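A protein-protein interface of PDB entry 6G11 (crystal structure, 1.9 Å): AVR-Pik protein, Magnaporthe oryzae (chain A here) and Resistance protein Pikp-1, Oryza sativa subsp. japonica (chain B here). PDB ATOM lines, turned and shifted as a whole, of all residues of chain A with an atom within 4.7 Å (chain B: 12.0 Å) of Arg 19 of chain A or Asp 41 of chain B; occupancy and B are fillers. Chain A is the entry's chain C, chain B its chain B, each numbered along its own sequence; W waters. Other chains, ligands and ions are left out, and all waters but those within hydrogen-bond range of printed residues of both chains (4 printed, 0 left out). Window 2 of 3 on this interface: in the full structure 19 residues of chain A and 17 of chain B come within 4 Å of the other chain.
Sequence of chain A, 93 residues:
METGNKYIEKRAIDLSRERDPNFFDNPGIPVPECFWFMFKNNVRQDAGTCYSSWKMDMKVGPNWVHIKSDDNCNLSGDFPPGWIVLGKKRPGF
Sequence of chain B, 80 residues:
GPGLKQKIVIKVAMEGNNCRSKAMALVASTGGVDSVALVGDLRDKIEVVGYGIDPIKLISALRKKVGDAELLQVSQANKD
OD1 of Asp 46 of chain A touches CA of Gly 40 of chain B (3.4 Å). Asp 41 of chain B touches Ala 47 of chain A (OD2 to N, 3.96 Å).
The side-chain carboxylate of Asp 41 of chain B lies within salt-bridge range of the guanidinium group of Arg 19 of chain A, at 3.8 Å. The guanidinium group (NE) of Arg 44 of chain A is in salt-bridge range of the side-chain carboxylate (OD2) of Asp 41 of chain B (2.8 Å). OD1 of Asp 46 of chain A lies within hydrogen-bond range of N of Asp 41 of chain B. OD1 of Asp 46 of chain A lies within salt-bridge range of NZ of Lys 45 of chain B (3.5 Å). The backbone carbonyl oxygen (O) of Ala 47 of chain A lies within hydrogen-bond range of the side-chain amino group (NZ) of Lys 45 of chain B (3.4 Å).
The side-chain carboxylate of Glu 18 of chain A is in salt-bridge range of the guanidinium group of Arg 44 of chain A. The backbone carbonyl oxygen (O) of Arg 19 of chain A is in hydrogen-bond range of the guanidinium group (NH1) of Arg 44 of chain A. The backbone NH (N) of Val 39 of chain B is in hydrogen-bond range of the backbone carbonyl oxygen (O) of Lys 45 of chain B (2.8 Å).
Printed residues of chain B within 4 Å of Arg 19 of chain A: Asp 41 (3.7 Å). Asp 20 of chain A touches none of the printed residues of chain B. No residue of chain B comes within 4 Å of Pro 21 of chain A. Asp 46 of chain A touches just these residues of chain B: Gly 40, Asp 41 and Lys 45. Of the printed residues of chain B, Ala 47 of chain A touches Asp 41 (3.96 Å) and Lys 45 (3.4 Å). Printed residues of chain A within 4 Å of Lys 45 of chain B: Asp 46 (3.2 Å) and Ala 47 (3.4 Å). Of the printed residues of chain A, Gly 40 of chain B touches Asp 46. Asp 44 of chain B touches none of the printed residues of chain A. The nearest residue of chain B that does not touch Arg 19 of chain A is Leu 42 of chain B (6.2 Å). The nearest printed residue of chain A that does not touch Lys 45 of chain B is Gln 45 of chain A (6.8 Å).
Water W3 lies within hydrogen-bond range of the side-chain carboxylate of Asp 44 of chain B, the side-chain carboxylate of Asp 46 of chain A, the backbone NH of Leu 42 of chain B and the backbone NH of Asp 41 of chain B. Water W1 bridges O of Ala 47 of chain A and N of Gly 40 of chain B. Water W2 bridges OD1 of Asp 41 of chain B (2.7 Å) and O of Ala 47 of chain A (3.2 Å). Water W4 lies within hydrogen-bond range of the side-chain carboxylate of Asp 41 of chain B (2.7 Å) and the backbone carbonyl oxygen of Gln 45 of chain A (3.4 Å).
Of the 10 printed residues of chain A, 4 touch a printed residue of chain B. Printed residues of chain A that touch a printed residue of chain B: Arg 19, Arg 44, Asp 46 and Ala 47. Of the 19 printed residues of chain B, 3 touch a printed residue of chain A. Printed residues of chain B that touch a printed residue of chain A: Gly 40, Asp 41 and Lys 45. Among the printed residues, Asp or Glu carboxylates within 4 Å of a Lys or Arg side-chain nitrogen of the other chain: Arg 19 of chain A with Asp 41 of chain B (3.8 Å), Arg 44 of chain A with Asp 41 of chain B (2.8 Å) and Asp 46 of chain A with Lys 45 of chain B (3.5 Å).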
ATOM      1  N   ARG A  17     -11.780  14.102  -2.552  1.00  0.00           N
ATOM      2  CA  ARG A  17     -11.344  15.332  -1.857  1.00  0.00           C
ATOM      3  C   ARG A  17     -10.064  15.917  -2.423  1.00  0.00           C
ATOM      4  O   ARG A  17      -9.562  16.891  -1.879  1.00  0.00           O
ATOM      5  CB  ARG A  17     -11.101  15.047  -0.371  1.00  0.00           C
ATOM      6  CG  ARG A  17     -12.082  14.076   0.297  1.00  0.00           C
ATOM      7  CD  ARG A  17     -13.315  14.710   0.839  1.00  0.00           C
ATOM      8  NE  ARG A  17     -12.939  15.805   1.707  1.00  0.00           N
ATOM      9  CZ  ARG A  17     -13.801  16.622   2.278  1.00  0.00           C
ATOM     10  NH1 ARG A  17     -15.122  16.436   2.147  1.00  0.00           N
ATOM     11  NH2 ARG A  17     -13.333  17.618   3.027  1.00  0.00           N
ATOM     12  N   GLU A  18      -9.525  15.350  -3.497  1.00  0.00           N
ATOM     13  CA  GLU A  18      -8.239  15.825  -4.001  1.00  0.00           C
ATOM     14  C   GLU A  18      -8.468  16.912  -5.010  1.00  0.00           C
ATOM     15  O   GLU A  18      -9.239  16.733  -5.918  1.00  0.00           O
ATOM     16  CB  GLU A  18      -7.435  14.686  -4.636  1.00  0.00           C
ATOM     17  CG  GLU A  18      -6.856  13.694  -3.644  1.00  0.00           C
ATOM     18  CD  GLU A  18      -5.823  14.300  -2.694  1.00  0.00           C
ATOM     19  OE1 GLU A  18      -5.201  15.338  -3.027  1.00  0.00           O
ATOM     20  OE2 GLU A  18      -5.637  13.732  -1.609  1.00  0.00           O
ATOM     21  N   ARG A  19      -7.739  18.010  -4.907  1.00  0.00           N
ATOM     22  CA  ARG A  19      -7.854  19.059  -5.908  1.00  0.00           C
ATOM     23  C   ARG A  19      -7.326  18.578  -7.242  1.00  0.00           C
ATOM     24  O   ARG A  19      -6.438  17.720  -7.305  1.00  0.00           O
ATOM     25  CB  ARG A  19      -7.157  20.362  -5.457  1.00  0.00           C
ATOM     26  CG  ARG A  19      -5.639  20.306  -5.502  1.00  0.00           C
ATOM     27  CD  ARG A  19      -5.033  21.475  -4.703  1.00  0.00           C
ATOM     28  NE  ARG A  19      -3.568  21.442  -4.709  1.00  0.00           N
ATOM     29  CZ  ARG A  19      -2.790  20.616  -3.995  1.00  0.00           C
ATOM     30  NH1 ARG A  19      -3.314  19.670  -3.209  1.00  0.00           N
ATOM     31  NH2 ARG A  19      -1.458  20.731  -4.077  1.00  0.00           N
ATOM     32  N   ASP A  20      -7.883  19.130  -8.313  1.00  0.00           N
ATOM     33  CA  ASP A  20      -7.466  18.791  -9.659  1.00  0.00           C
ATOM     34  C   ASP A  20      -5.972  19.139  -9.862  1.00  0.00           C
ATOM     35  O   ASP A  20      -5.466  20.073  -9.261  1.00  0.00           O
ATOM     36  CB  ASP A  20      -8.302  19.525 -10.728  1.00  0.00           C
ATOM     37  CG  ASP A  20      -9.698  18.942 -10.899  1.00  0.00           C
ATOM     38  OD1 ASP A  20     -10.097  17.946 -10.269  1.00  0.00           O
ATOM     39  OD2 ASP A  20     -10.415  19.470 -11.720  1.00  0.00           O
ATOM     40  N   PRO A  21      -5.280  18.366 -10.675  1.00  0.00           N
ATOM     41  CA  PRO A  21      -3.903  18.708 -11.028  1.00  0.00           C
ATOM     42  C   PRO A  21      -3.806  20.000 -11.839  1.00  0.00           C
ATOM     43  O   PRO A  21      -4.768  20.384 -12.494  1.00  0.00           O
ATOM     44  CB  PRO A  21      -3.450  17.561 -11.930  1.00  0.00           C
ATOM     45  CG  PRO A  21      -4.471  16.504 -11.780  1.00  0.00           C
ATOM     46  CD  PRO A  21      -5.729  17.119 -11.293  1.00  0.00           C
ATOM     47  N   PHE A  37      -2.766  10.740  -9.542  1.00  0.00           N
ATOM     48  CA  PHE A  37      -2.346  11.302  -8.263  1.00  0.00           C
ATOM     49  C   PHE A  37      -1.349  10.342  -7.617  1.00  0.00           C
ATOM     50  O   PHE A  37      -1.634   9.155  -7.463  1.00  0.00           O
ATOM     51  CB  PHE A  37      -3.582  11.482  -7.329  1.00  0.00           C
ATOM     52  CG  PHE A  37      -4.672  12.335  -7.910  1.00  0.00           C
ATOM     53  CD1 PHE A  37      -5.636  11.780  -8.745  1.00  0.00           C
ATOM     54  CD2 PHE A  37      -4.735  13.675  -7.622  1.00  0.00           C
ATOM     55  CE1 PHE A  37      -6.648  12.554  -9.275  1.00  0.00           C
ATOM     56  CE2 PHE A  37      -5.735  14.460  -8.142  1.00  0.00           C
ATOM     57  CZ  PHE A  37      -6.704  13.898  -8.955  1.00  0.00           C
ATOM     58  N   ARG A  44      -0.027  13.198  -0.639  1.00  0.00           N
ATOM     59  CA  ARG A  44       0.014  13.544  -2.054  1.00  0.00           C
ATOM     60  C   ARG A  44       1.364  14.138  -2.408  1.00  0.00           C
ATOM     61  O   ARG A  44       1.759  15.094  -1.797  1.00  0.00           O
ATOM     62  CB  ARG A  44      -1.062  14.579  -2.366  1.00  0.00           C
ATOM     63  CG  ARG A  44      -1.003  15.124  -3.792  1.00  0.00           C
ATOM     64  CD  ARG A  44      -2.280  15.804  -4.163  1.00  0.00           C
ATOM     65  NE  ARG A  44      -2.250  16.606  -5.387  1.00  0.00           N
ATOM     66  CZ  ARG A  44      -3.353  17.038  -6.000  1.00  0.00           C
ATOM     67  NH1 ARG A  44      -4.570  16.732  -5.536  1.00  0.00           N
ATOM     68  NH2 ARG A  44      -3.243  17.791  -7.057  1.00  0.00           N
ATOM     69  N   GLN A  45       2.064  13.563  -3.388  1.00  0.00           N
ATOM     70  CA  GLN A  45       3.315  14.111  -3.844  1.00  0.00           C
ATOM     71  C   GLN A  45       3.140  15.005  -5.081  1.00  0.00           C
ATOM     72  O   GLN A  45       3.763  16.048  -5.203  1.00  0.00           O
ATOM     73  CB  GLN A  45       4.269  12.968  -4.142  1.00  0.00           C
ATOM     74  CG  GLN A  45       4.464  12.019  -2.963  1.00  0.00           C
ATOM     75  CD  GLN A  45       5.157  12.715  -1.831  1.00  0.00           C
ATOM     76  OE1 GLN A  45       6.280  13.162  -1.975  1.00  0.00           O
ATOM     77  NE2 GLN A  45       4.457  12.867  -0.710  1.00  0.00           N
ATOM     78  N   ASP A  46       2.308  14.577  -6.015  1.00  0.00           N
ATOM     79  CA  ASP A  46       2.027  15.368  -7.207  1.00  0.00           C
ATOM     80  C   ASP A  46       0.905  14.711  -7.970  1.00  0.00           C
ATOM     81  O   ASP A  46       0.371  13.669  -7.537  1.00  0.00           O
ATOM     82  CB  ASP A  46       3.267  15.561  -8.110  1.00  0.00           C
ATOM     83  CG  ASP A  46       3.335  16.971  -8.685  1.00  0.00           C
ATOM     84  OD1 ASP A  46       2.278  17.546  -9.082  1.00  0.00           O
ATOM     85  OD2 ASP A  46       4.446  17.517  -8.748  1.00  0.00           O
ATOM     86  N   ALA A  47       0.535  15.343  -9.085  1.00  0.00           N
ATOM     87  CA  ALA A  47      -0.559  14.863  -9.902  1.00  0.00           C
ATOM     88  C   ALA A  47      -0.413  15.376 -11.348  1.00  0.00           C
ATOM     89  O   ALA A  47       0.322  16.348 -11.626  1.00  0.00           O
ATOM     90  CB  ALA A  47      -1.864  15.314  -9.287  1.00  0.00           C
ATOM     91  N   VAL B   9       8.213  14.736 -19.247  1.00  0.00           N
ATOM     92  CA  VAL B   9       8.042  15.625 -18.070  1.00  0.00           C
ATOM     93  C   VAL B   9       9.348  15.707 -17.280  1.00  0.00           C
ATOM     94  O   VAL B   9       9.938  14.662 -16.955  1.00  0.00           O
ATOM     95  CB  VAL B   9       6.888  15.208 -17.172  1.00  0.00           C
ATOM     96  CG1 VAL B   9       6.727  16.153 -16.010  1.00  0.00           C
ATOM     97  CG2 VAL B   9       5.581  15.143 -17.946  1.00  0.00           C
ATOM     98  N   ILE B  10       9.814  16.925 -17.025  1.00  0.00           N
ATOM     99  CA  ILE B  10      11.065  17.170 -16.323  1.00  0.00           C
ATOM    100  C   ILE B  10      10.841  18.072 -15.108  1.00  0.00           C
ATOM    101  O   ILE B  10      10.211  19.102 -15.223  1.00  0.00           O
ATOM    102  CB  ILE B  10      12.055  17.857 -17.252  1.00  0.00           C
ATOM    103  CG1 ILE B  10      12.387  16.893 -18.418  1.00  0.00           C
ATOM    104  CG2 ILE B  10      13.329  18.251 -16.502  1.00  0.00           C
ATOM    105  CD1 ILE B  10      13.280  17.469 -19.488  1.00  0.00           C
ATOM    106  N   LYS B  11      11.342  17.672 -13.939  1.00  0.00           N
ATOM    107  CA  LYS B  11      11.335  18.527 -12.758  1.00  0.00           C
ATOM    108  C   LYS B  11      12.588  19.364 -12.748  1.00  0.00           C
ATOM    109  O   LYS B  11      13.653  18.835 -12.924  1.00  0.00           O
ATOM    110  CB  LYS B  11      11.265  17.693 -11.494  1.00  0.00           C
ATOM    111  CG  LYS B  11      11.159  18.549 -10.234  1.00  0.00           C
ATOM    112  CD  LYS B  11      11.333  17.710  -9.002  1.00  0.00           C
ATOM    113  CE  LYS B  11       9.982  17.195  -8.520  1.00  0.00           C
ATOM    114  NZ  LYS B  11       9.052  18.303  -8.154  1.00  0.00           N
ATOM    115  N   VAL B  12      12.476  20.670 -12.551  1.00  0.00           N
ATOM    116  CA  VAL B  12      13.669  21.545 -12.485  1.00  0.00           C
ATOM    117  C   VAL B  12      13.697  22.267 -11.126  1.00  0.00           C
ATOM    118  O   VAL B  12      12.638  22.614 -10.578  1.00  0.00           O
ATOM    119  CB  VAL B  12      13.718  22.544 -13.672  1.00  0.00           C
ATOM    120  CG1 VAL B  12      13.797  21.819 -15.015  1.00  0.00           C
ATOM    121  CG2 VAL B  12      12.529  23.411 -13.730  1.00  0.00           C
ATOM    122  N   MET B  14      14.066  25.321  -8.602  1.00  0.00           N
ATOM    123  CA  MET B  14      13.682  26.758  -8.698  1.00  0.00           C
ATOM    124  C   MET B  14      14.029  27.534  -7.435  1.00  0.00           C
ATOM    125  O   MET B  14      15.126  28.072  -7.317  1.00  0.00           O
ATOM    126  CB  MET B  14      12.169  26.887  -8.963  1.00  0.00           C
ATOM    127  CG  MET B  14      11.573  25.910  -9.980  1.00  0.00           C
ATOM    128  SD  MET B  14      12.054  26.160 -11.722  1.00  0.00           S
ATOM    129  CE  MET B  14      10.587  25.438 -12.534  1.00  0.00           C
ATOM    130  N   ARG B  20      12.840  29.249 -13.818  1.00  0.00           N
ATOM    131  CA  ARG B  20      11.623  28.805 -14.510  1.00  0.00           C
ATOM    132  C   ARG B  20      11.673  29.237 -15.966  1.00  0.00           C
ATOM    133  O   ARG B  20      11.570  28.399 -16.876  1.00  0.00           O
ATOM    134  CB  ARG B  20      10.333  29.359 -13.869  1.00  0.00           C
ATOM    135  CG  ARG B  20       9.626  28.353 -13.012  1.00  0.00           C
ATOM    136  CD  ARG B  20       8.345  28.765 -12.273  1.00  0.00           C
ATOM    137  NE  ARG B  20       8.063  27.772 -11.245  1.00  0.00           N
ATOM    138  CZ  ARG B  20       8.450  27.830  -9.963  1.00  0.00           C
ATOM    139  NH1 ARG B  20       8.176  26.805  -9.150  1.00  0.00           N
ATOM    140  NH2 ARG B  20       9.156  28.849  -9.482  1.00  0.00           N
ATOM    141  N   ALA B  37       4.933  23.470 -21.154  1.00  0.00           N
ATOM    142  CA  ALA B  37       4.014  23.971 -20.169  1.00  0.00           C
ATOM    143  C   ALA B  37       4.549  23.690 -18.770  1.00  0.00           C
ATOM    144  O   ALA B  37       5.048  22.571 -18.512  1.00  0.00           O
ATOM    145  CB  ALA B  37       2.644  23.325 -20.335  1.00  0.00           C
ATOM    146  N   LEU B  38       4.412  24.676 -17.892  1.00  0.00           N
ATOM    147  CA  LEU B  38       4.713  24.498 -16.480  1.00  0.00           C
ATOM    148  C   LEU B  38       3.558  23.822 -15.841  1.00  0.00           C
ATOM    149  O   LEU B  38       2.493  24.322 -15.909  1.00  0.00           O
ATOM    150  CB  LEU B  38       4.925  25.829 -15.786  1.00  0.00           C
ATOM    151  CG  LEU B  38       6.205  26.531 -16.078  1.00  0.00           C
ATOM    152  CD1 LEU B  38       6.115  27.950 -15.479  1.00  0.00           C
ATOM    153  CD2 LEU B  38       7.383  25.719 -15.508  1.00  0.00           C
ATOM    154  N   VAL B  39       3.777  22.674 -15.225  1.00  0.00           N
ATOM    155  CA  VAL B  39       2.702  21.901 -14.631  1.00  0.00           C
ATOM    156  C   VAL B  39       3.144  21.449 -13.228  1.00  0.00           C
ATOM    157  O   VAL B  39       4.261  21.755 -12.769  1.00  0.00           O
ATOM    158  CB  VAL B  39       2.332  20.671 -15.529  1.00  0.00           C
ATOM    159  CG1 VAL B  39       1.733  21.163 -16.842  1.00  0.00           C
ATOM    160  CG2 VAL B  39       3.506  19.703 -15.699  1.00  0.00           C
ATOM    161  N   GLY B  40       2.268  20.695 -12.582  1.00  0.00           N
ATOM    162  CA  GLY B  40       2.586  20.087 -11.310  1.00  0.00           C
ATOM    163  C   GLY B  40       2.064  20.924 -10.176  1.00  0.00           C
ATOM    164  O   GLY B  40       1.876  22.145 -10.310  1.00  0.00           O
ATOM    165  N   ASP B  41       1.858  20.260  -9.037  1.00  0.00           N
ATOM    166  CA  ASP B  41       1.301  20.897  -7.843  1.00  0.00           C
ATOM    167  C   ASP B  41       2.150  22.109  -7.451  1.00  0.00           C
ATOM    168  O   ASP B  41       1.613  23.096  -7.046  1.00  0.00           O
ATOM    169  CB  ASP B  41       1.240  19.868  -6.692  1.00  0.00           C
ATOM    170  CG  ASP B  41       0.116  18.852  -6.860  1.00  0.00           C
ATOM    171  OD1 ASP B  41      -0.770  18.935  -7.772  1.00  0.00           O
ATOM    172  OD2 ASP B  41       0.121  17.888  -6.078  1.00  0.00           O
ATOM    173  N   LEU B  42       3.469  22.046  -7.607  1.00  0.00           N
ATOM    174  CA  LEU B  42       4.338  23.194  -7.237  1.00  0.00           C
ATOM    175  C   LEU B  42       4.774  24.037  -8.423  1.00  0.00           C
ATOM    176  O   LEU B  42       5.673  24.891  -8.324  1.00  0.00           O
ATOM    177  CB  LEU B  42       5.552  22.729  -6.442  1.00  0.00           C
ATOM    178  CG  LEU B  42       5.207  22.032  -5.108  1.00  0.00           C
ATOM    179  CD1 LEU B  42       6.434  21.423  -4.458  1.00  0.00           C
ATOM    180  CD2 LEU B  42       4.454  22.946  -4.135  1.00  0.00           C
ATOM    181  N   ARG B  43       4.211  23.746  -9.588  1.00  0.00           N
ATOM    182  CA  ARG B  43       4.568  24.469 -10.793  1.00  0.00           C
ATOM    183  C   ARG B  43       6.066  24.428 -11.040  1.00  0.00           C
ATOM    184  O   ARG B  43       6.665  25.383 -11.491  1.00  0.00           O
ATOM    185  CB  ARG B  43       3.947  25.875 -10.772  1.00  0.00           C
ATOM    186  CG  ARG B  43       2.412  25.794 -10.812  1.00  0.00           C
ATOM    187  CD  ARG B  43       1.684  27.142 -10.785  1.00  0.00           C
ATOM    188  NE  ARG B  43       1.879  27.875 -12.054  1.00  0.00           N
ATOM    189  CZ  ARG B  43       2.886  28.713 -12.318  1.00  0.00           C
ATOM    190  NH1 ARG B  43       3.817  29.011 -11.405  1.00  0.00           N
ATOM    191  NH2 ARG B  43       2.977  29.275 -13.516  1.00  0.00           N
ATOM    192  N   ASP B  44       6.646  23.254 -10.806  1.00  0.00           N
ATOM    193  CA  ASP B  44       8.083  23.123 -10.951  1.00  0.00           C
ATOM    194  C   ASP B  44       8.470  22.049 -11.977  1.00  0.00           C
ATOM    195  O   ASP B  44       9.629  21.611 -12.022  1.00  0.00           O
ATOM    196  CB  ASP B  44       8.739  22.836  -9.581  1.00  0.00           C
ATOM    197  CG  ASP B  44       8.231  21.550  -8.949  1.00  0.00           C
ATOM    198  OD1 ASP B  44       7.208  20.971  -9.400  1.00  0.00           O
ATOM    199  OD2 ASP B  44       8.913  21.094  -8.029  1.00  0.00           O
ATOM    200  N   LYS B  45       7.509  21.604 -12.763  1.00  0.00           N
ATOM    201  CA  LYS B  45       7.735  20.612 -13.799  1.00  0.00           C
ATOM    202  C   LYS B  45       7.434  21.248 -15.185  1.00  0.00           C
ATOM    203  O   LYS B  45       6.524  22.049 -15.312  1.00  0.00           O
ATOM    204  CB  LYS B  45       6.838  19.395 -13.580  1.00  0.00           C
ATOM    205  CG  LYS B  45       7.144  18.578 -12.334  1.00  0.00           C
ATOM    206  CD  LYS B  45       6.185  17.352 -12.289  1.00  0.00           C
ATOM    207  CE  LYS B  45       4.712  17.602 -11.974  1.00  0.00           C
ATOM    208  NZ  LYS B  45       3.748  16.434 -12.016  1.00  0.00           N
ATOM    209  N   ILE B  46       8.217  20.854 -16.170  1.00  0.00           N
ATOM    210  CA  ILE B  46       7.986  21.208 -17.548  1.00  0.00           C
ATOM    211  C   ILE B  46       7.534  19.967 -18.314  1.00  0.00           C
ATOM    212  O   ILE B  46       8.238  18.946 -18.311  1.00  0.00           O
ATOM    213  CB  ILE B  46       9.238  21.790 -18.194  1.00  0.00           C
ATOM    214  CG1 ILE B  46       9.633  23.039 -17.426  1.00  0.00           C
ATOM    215  CG2 ILE B  46       8.952  22.110 -19.681  1.00  0.00           C
ATOM    216  CD1 ILE B  46      10.816  23.758 -17.988  1.00  0.00           C
ATOM    217  N   GLU B  47       6.340  20.077 -18.898  1.00  0.00           N
ATOM    218  CA  GLU B  47       5.778  19.076 -19.778  1.00  0.00           C
ATOM    219  C   GLU B  47       6.011  19.520 -21.225  1.00  0.00           C
ATOM    220  O   GLU B  47       5.571  20.612 -21.614  1.00  0.00           O
ATOM    221  CB  GLU B  47       4.282  18.869 -19.479  1.00  0.00           C
ATOM    222  CG  GLU B  47       3.689  17.809 -20.373  1.00  0.00           C
ATOM    223  CD  GLU B  47       2.246  17.431 -20.024  1.00  0.00           C
ATOM    224  OE1 GLU B  47       1.438  17.394 -20.975  1.00  0.00           O
ATOM    225  OE2 GLU B  47       1.892  17.183 -18.863  1.00  0.00           O
ATOM    226  N   LEU B  72      11.139  12.790 -15.194  1.00  0.00           N
ATOM    227  CA  LEU B  72      10.073  12.137 -14.459  1.00  0.00           C
ATOM    228  C   LEU B  72       9.142  11.268 -15.273  1.00  0.00           C
ATOM    229  O   LEU B  72       8.508  10.375 -14.699  1.00  0.00           O
ATOM    230  CB  LEU B  72       9.236  13.181 -13.740  1.00  0.00           C
ATOM    231  CG  LEU B  72       9.885  13.987 -12.641  1.00  0.00           C
ATOM    232  CD1 LEU B  72       8.813  14.855 -11.997  1.00  0.00           C
ATOM    233  CD2 LEU B  72      10.550  13.135 -11.582  1.00  0.00           C
ATOM    234  N   GLN B  73       8.991  11.560 -16.566  1.00  0.00           N
ATOM    235  CA  GLN B  73       7.993  10.849 -17.363  1.00  0.00           C
ATOM    236  C   GLN B  73       8.429  10.911 -18.814  1.00  0.00           C
ATOM    237  O   GLN B  73       8.914  11.956 -19.304  1.00  0.00           O
ATOM    238  CB  GLN B  73       6.607  11.454 -17.206  1.00  0.00           C
ATOM    239  CG  GLN B  73       5.511  10.638 -17.781  1.00  0.00           C
ATOM    240  CD  GLN B  73       4.133  11.293 -17.681  1.00  0.00           C
ATOM    241  OE1 GLN B  73       3.802  11.973 -16.682  1.00  0.00           O
ATOM    242  NE2 GLN B  73       3.324  11.123 -18.753  1.00  0.00           N
HETATM  243  O   HOH W   1       0.641  18.148 -13.499  1.00  0.00           O
HETATM  244  O   HOH W   2      -0.614  19.128 -10.446  1.00  0.00           O
HETATM  245  O   HOH W   3       5.019  20.051  -8.785  1.00  0.00           O
HETATM  246  O   HOH W   4       1.442  18.000  -3.739  1.00  0.00           O
